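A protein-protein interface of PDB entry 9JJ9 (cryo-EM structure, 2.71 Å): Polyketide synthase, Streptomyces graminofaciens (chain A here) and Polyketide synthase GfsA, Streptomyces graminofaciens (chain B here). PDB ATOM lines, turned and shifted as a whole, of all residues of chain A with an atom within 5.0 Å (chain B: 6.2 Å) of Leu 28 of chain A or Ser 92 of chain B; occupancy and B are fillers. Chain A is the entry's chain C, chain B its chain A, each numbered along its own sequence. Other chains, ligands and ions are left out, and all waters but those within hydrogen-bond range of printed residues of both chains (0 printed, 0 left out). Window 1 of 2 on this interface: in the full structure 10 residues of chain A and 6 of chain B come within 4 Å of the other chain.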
ATOM      1  N   ALA A  25     -33.932 -14.820 -12.870  1.00  0.00           N
ATOM      2  CA  ALA A  25     -33.447 -14.772 -14.244  1.00  0.00           C
ATOM      3  C   ALA A  25     -32.314 -15.757 -14.505  1.00  0.00           C
ATOM      4  O   ALA A  25     -31.929 -15.939 -15.665  1.00  0.00           O
ATOM      5  CB  ALA A  25     -32.988 -13.354 -14.588  1.00  0.00           C
ATOM      6  N   HIS A  26     -31.789 -16.408 -13.464  1.00  0.00           N
ATOM      7  CA  HIS A  26     -30.658 -17.318 -13.600  1.00  0.00           C
ATOM      8  C   HIS A  26     -31.025 -18.535 -14.440  1.00  0.00           C
ATOM      9  O   HIS A  26     -30.146 -19.300 -14.851  1.00  0.00           O
ATOM     10  CB  HIS A  26     -30.158 -17.760 -12.224  1.00  0.00           C
ATOM     11  CG  HIS A  26     -30.915 -18.917 -11.649  1.00  0.00           C
ATOM     12  ND1 HIS A  26     -32.264 -18.861 -11.374  1.00  0.00           N
ATOM     13  CD2 HIS A  26     -30.511 -20.161 -11.299  1.00  0.00           C
ATOM     14  CE1 HIS A  26     -32.659 -20.021 -10.879  1.00  0.00           C
ATOM     15  NE2 HIS A  26     -31.614 -20.827 -10.824  1.00  0.00           N
ATOM     16  N   VAL A  27     -32.323 -18.725 -14.697  1.00  0.00           N
ATOM     17  CA  VAL A  27     -32.762 -19.780 -15.600  1.00  0.00           C
ATOM     18  C   VAL A  27     -32.226 -19.560 -17.008  1.00  0.00           C
ATOM     19  O   VAL A  27     -32.178 -20.501 -17.807  1.00  0.00           O
ATOM     20  CB  VAL A  27     -34.304 -19.879 -15.597  1.00  0.00           C
ATOM     21  CG1 VAL A  27     -34.917 -18.791 -16.469  1.00  0.00           C
ATOM     22  CG2 VAL A  27     -34.753 -21.260 -16.055  1.00  0.00           C
ATOM     23  N   LEU A  28     -31.817 -18.331 -17.336  1.00  0.00           N
ATOM     24  CA  LEU A  28     -31.219 -18.068 -18.638  1.00  0.00           C
ATOM     25  C   LEU A  28     -29.787 -18.578 -18.733  1.00  0.00           C
ATOM     26  O   LEU A  28     -29.244 -18.661 -19.840  1.00  0.00           O
ATOM     27  CB  LEU A  28     -31.261 -16.572 -18.944  1.00  0.00           C
ATOM     28  CG  LEU A  28     -32.628 -16.041 -19.377  1.00  0.00           C
ATOM     29  CD1 LEU A  28     -32.959 -14.744 -18.654  1.00  0.00           C
ATOM     30  CD2 LEU A  28     -32.674 -15.859 -20.885  1.00  0.00           C
ATOM     31  N   GLY A  29     -29.167 -18.917 -17.607  1.00  0.00           N
ATOM     32  CA  GLY A  29     -27.816 -19.440 -17.613  1.00  0.00           C
ATOM     33  C   GLY A  29     -26.716 -18.406 -17.625  1.00  0.00           C
ATOM     34  O   GLY A  29     -25.578 -18.742 -17.973  1.00  0.00           O
ATOM     35  N   LEU A  30     -27.009 -17.161 -17.261  1.00  0.00           N
ATOM     36  CA  LEU A  30     -25.997 -16.105 -17.227  1.00  0.00           C
ATOM     37  C   LEU A  30     -25.327 -16.015 -15.859  1.00  0.00           C
ATOM     38  O   LEU A  30     -25.228 -14.941 -15.266  1.00  0.00           O
ATOM     39  CB  LEU A  30     -26.625 -14.771 -17.615  1.00  0.00           C
ATOM     40  CG  LEU A  30     -26.458 -14.316 -19.066  1.00  0.00           C
ATOM     41  CD1 LEU A  30     -24.988 -14.301 -19.462  1.00  0.00           C
ATOM     42  CD2 LEU A  30     -27.264 -15.197 -20.006  1.00  0.00           C
ATOM     43  N   VAL A  36     -27.709 -10.181 -16.162  1.00  0.00           N
ATOM     44  CA  VAL A  36     -28.975  -9.942 -16.842  1.00  0.00           C
ATOM     45  C   VAL A  36     -29.233  -8.443 -16.915  1.00  0.00           C
ATOM     46  O   VAL A  36     -29.044  -7.712 -15.934  1.00  0.00           O
ATOM     47  CB  VAL A  36     -30.119 -10.681 -16.130  1.00  0.00           C
ATOM     48  CG1 VAL A  36     -30.000 -12.178 -16.365  1.00  0.00           C
ATOM     49  CG2 VAL A  36     -30.108 -10.375 -14.638  1.00  0.00           C
ATOM     50  N   LEU A  45     -32.489 -11.853 -26.102  1.00  0.00           N
ATOM     51  CA  LEU A  45     -31.686 -12.562 -25.115  1.00  0.00           C
ATOM     52  C   LEU A  45     -32.020 -14.049 -25.064  1.00  0.00           C
ATOM     53  O   LEU A  45     -31.238 -14.832 -24.513  1.00  0.00           O
ATOM     54  CB  LEU A  45     -31.873 -11.900 -23.744  1.00  0.00           C
ATOM     55  CG  LEU A  45     -31.336 -12.537 -22.461  1.00  0.00           C
ATOM     56  CD1 LEU A  45     -29.982 -11.950 -22.105  1.00  0.00           C
ATOM     57  CD2 LEU A  45     -32.322 -12.312 -21.329  1.00  0.00           C
ATOM     58  N   GLY A  46     -33.142 -14.458 -25.651  1.00  0.00           N
ATOM     59  CA  GLY A  46     -33.496 -15.861 -25.726  1.00  0.00           C
ATOM     60  C   GLY A  46     -34.637 -16.257 -24.812  1.00  0.00           C
ATOM     61  O   GLY A  46     -34.438 -16.462 -23.612  1.00  0.00           O
ATOM     62  N   PHE A  47     -35.840 -16.378 -25.375  1.00  0.00           N
ATOM     63  CA  PHE A  47     -37.015 -16.762 -24.597  1.00  0.00           C
ATOM     64  C   PHE A  47     -38.033 -17.379 -25.547  1.00  0.00           C
ATOM     65  O   PHE A  47     -38.627 -16.667 -26.361  1.00  0.00           O
ATOM     66  CB  PHE A  47     -37.605 -15.560 -23.868  1.00  0.00           C
ATOM     67  CG  PHE A  47     -37.326 -15.543 -22.393  1.00  0.00           C
ATOM     68  CD1 PHE A  47     -38.082 -16.312 -21.523  1.00  0.00           C
ATOM     69  CD2 PHE A  47     -36.313 -14.756 -21.873  1.00  0.00           C
ATOM     70  CE1 PHE A  47     -37.831 -16.299 -20.165  1.00  0.00           C
ATOM     71  CE2 PHE A  47     -36.056 -14.738 -20.515  1.00  0.00           C
ATOM     72  CZ  PHE A  47     -36.818 -15.511 -19.660  1.00  0.00           C
ATOM     73  N   ALA B  86     -22.099 -17.350 -28.606  1.00  0.00           N
ATOM     74  CA  ALA B  86     -23.552 -17.468 -28.636  1.00  0.00           C
ATOM     75  C   ALA B  86     -24.249 -16.113 -28.615  1.00  0.00           C
ATOM     76  O   ALA B  86     -25.388 -16.011 -29.082  1.00  0.00           O
ATOM     77  CB  ALA B  86     -24.034 -18.318 -27.460  1.00  0.00           C
ATOM     78  N   GLY B  90     -27.670 -14.567 -30.823  1.00  0.00           N
ATOM     79  CA  GLY B  90     -28.828 -14.492 -29.948  1.00  0.00           C
ATOM     80  C   GLY B  90     -29.262 -15.824 -29.374  1.00  0.00           C
ATOM     81  O   GLY B  90     -30.462 -16.126 -29.356  1.00  0.00           O
ATOM     82  N   ILE B  91     -28.314 -16.630 -28.906  1.00  0.00           N
ATOM     83  CA  ILE B  91     -28.590 -17.951 -28.354  1.00  0.00           C
ATOM     84  C   ILE B  91     -28.187 -17.946 -26.886  1.00  0.00           C
ATOM     85  O   ILE B  91     -27.079 -17.519 -26.543  1.00  0.00           O
ATOM     86  CB  ILE B  91     -27.845 -19.054 -29.127  1.00  0.00           C
ATOM     87  CG1 ILE B  91     -28.462 -19.236 -30.515  1.00  0.00           C
ATOM     88  CG2 ILE B  91     -27.870 -20.365 -28.355  1.00  0.00           C
ATOM     89  CD1 ILE B  91     -27.686 -20.172 -31.412  1.00  0.00           C
ATOM     90  N   SER B  92     -29.090 -18.410 -26.025  1.00  0.00           N
ATOM     91  CA  SER B  92     -28.816 -18.434 -24.598  1.00  0.00           C
ATOM     92  C   SER B  92     -27.691 -19.420 -24.285  1.00  0.00           C
ATOM     93  O   SER B  92     -27.529 -20.430 -24.974  1.00  0.00           O
ATOM     94  CB  SER B  92     -30.073 -18.816 -23.820  1.00  0.00           C
ATOM     95  OG  SER B  92     -31.072 -17.818 -23.943  1.00  0.00           O
ATOM     96  N   PRO B  93     -26.887 -19.136 -23.253  1.00  0.00           N
ATOM     97  CA  PRO B  93     -25.801 -20.068 -22.900  1.00  0.00           C
ATOM     98  C   PRO B  93     -26.290 -21.462 -22.548  1.00  0.00           C
ATOM     99  O   PRO B  93     -25.601 -22.446 -22.842  1.00  0.00           O
ATOM    100  CB  PRO B  93     -25.129 -19.380 -21.703  1.00  0.00           C
ATOM    101  CG  PRO B  93     -25.483 -17.935 -21.843  1.00  0.00           C
ATOM    102  CD  PRO B  93     -26.859 -17.912 -22.437  1.00  0.00           C
ATOM    103  N   ARG B  94     -27.462 -21.574 -21.915  1.00  0.00           N
ATOM    104  CA  ARG B  94     -28.001 -22.891 -21.592  1.00  0.00           C
ATOM    105  C   ARG B  94     -28.296 -23.691 -22.855  1.00  0.00           C
ATOM    106  O   ARG B  94     -28.003 -24.890 -22.923  1.00  0.00           O
ATOM    107  CB  ARG B  94     -29.260 -22.749 -20.737  1.00  0.00           C
ATOM    108  CG  ARG B  94     -29.606 -23.992 -19.934  1.00  0.00           C
ATOM    109  CD  ARG B  94     -30.890 -23.800 -19.144  1.00  0.00           C
ATOM    110  NE  ARG B  94     -32.074 -24.054 -19.956  1.00  0.00           N
ATOM    111  CZ  ARG B  94     -33.321 -23.979 -19.510  1.00  0.00           C
ATOM    112  NH1 ARG B  94     -33.586 -23.659 -18.253  1.00  0.00           N
ATOM    113  NH2 ARG B  94     -34.325 -24.232 -20.343  1.00  0.00           N
ATOM    114  N   GLU B  95     -28.884 -23.044 -23.864  1.00  0.00           N
ATOM    115  CA  GLU B  95     -29.132 -23.720 -25.133  1.00  0.00           C
ATOM    116  C   GLU B  95     -27.825 -24.060 -25.841  1.00  0.00           C
ATOM    117  O   GLU B  95     -27.699 -25.134 -26.440  1.00  0.00           O
ATOM    118  CB  GLU B  95     -30.020 -22.851 -26.024  1.00  0.00           C
ATOM    119  CG  GLU B  95     -30.212 -23.387 -27.433  1.00  0.00           C
ATOM    120  CD  GLU B  95     -31.039 -22.459 -28.301  1.00  0.00           C
ATOM    121  OE1 GLU B  95     -31.089 -21.248 -28.001  1.00  0.00           O
ATOM    122  OE2 GLU B  95     -31.642 -22.942 -29.284  1.00  0.00           O
ATOM    123  N   ALA B  96     -26.843 -23.157 -25.781  1.00  0.00           N
ATOM    124  CA  ALA B  96     -25.562 -23.407 -26.433  1.00  0.00           C
ATOM    125  C   ALA B  96     -24.799 -24.547 -25.770  1.00  0.00           C
ATOM    126  O   ALA B  96     -24.004 -25.223 -26.433  1.00  0.00           O
ATOM    127  CB  ALA B  96     -24.716 -22.133 -26.435  1.00  0.00           C
ATOM    128  N   ALA B  97     -25.018 -24.768 -24.471  1.00  0.00           N
ATOM    129  CA  ALA B  97     -24.329 -25.854 -23.779  1.00  0.00           C
ATOM    130  C   ALA B  97     -24.711 -27.209 -24.358  1.00  0.00           C
ATOM    131  O   ALA B  97     -23.849 -28.073 -24.558  1.00  0.00           O
ATOM    132  CB  ALA B  97     -24.637 -25.801 -22.283  1.00  0.00           C
ATOM    133  N   HIS B 594     -18.631 -23.589 -24.144  1.00  0.00           N
ATOM    134  CA  HIS B 594     -19.994 -24.087 -23.958  1.00  0.00           C
ATOM    135  C   HIS B 594     -19.956 -25.601 -24.148  1.00  0.00           C
ATOM    136  O   HIS B 594     -19.928 -26.089 -25.282  1.00  0.00           O
ATOM    137  CB  HIS B 594     -20.967 -23.428 -24.930  1.00  0.00           C
ATOM    138  CG  HIS B 594     -21.180 -21.969 -24.675  1.00  0.00           C
ATOM    139  ND1 HIS B 594     -20.886 -21.001 -25.612  1.00  0.00           N
ATOM    140  CD2 HIS B 594     -21.660 -21.312 -23.593  1.00  0.00           C
ATOM    141  CE1 HIS B 594     -21.174 -19.811 -25.116  1.00  0.00           C
ATOM    142  NE2 HIS B 594     -21.644 -19.972 -23.893  1.00  0.00           N
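Among the printed residues, merely in contact across the chains: Leu 28 of chain A with Ser 92 of chain B, Leu 28 of chain A with Pro 93 of chain B, Leu 28 of chain A with Arg 94 of chain B, Gly 29 of chain A with Pro 93 of chain B, Leu 30 of chain A with Pro 93 of chain B and Gly 46 of chain A with Ser 92 of chain B.
Of chain A, only Leu 28 (3.97 Å), Leu 45 (3.0 Å) and Gly 46 (3.6 Å) come within 4 Å of Ser 92 of chain B. Printed residues of chain B within 4 Å of Gly 46 of chain A: Ser 92. Of the printed residues of chain A, Arg 94 of chain B touches Val 27 and Leu 28. Printed residues of chain A within 4 Å of Pro 93 of chain B: Leu 28, Gly 29 and Leu 30. The nearest printed residue of chain A that does not touch Ser 92 of chain B is Phe 47 of chain A (5.2 Å).
Of the 10 printed residues of chain B, 3 touch a printed residue of chain A. Along chain B the printed residues that touch a printed residue of chain A span positions 92 to 94. Among the printed residues, 8 pairs touch across the chains. Among the printed residues, no Asp or Glu carboxylate lies within 4 Å of a Lys or Arg side-chain nitrogen of the other chain.
OG of Ser 92 of chain B sits at hydrogen-bond distance from O of Leu 45 of chain A, 3.0 Å away. NH1 of Arg 94 of chain B sits close to O of Val 27 of chain A, 3.5 Å away.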
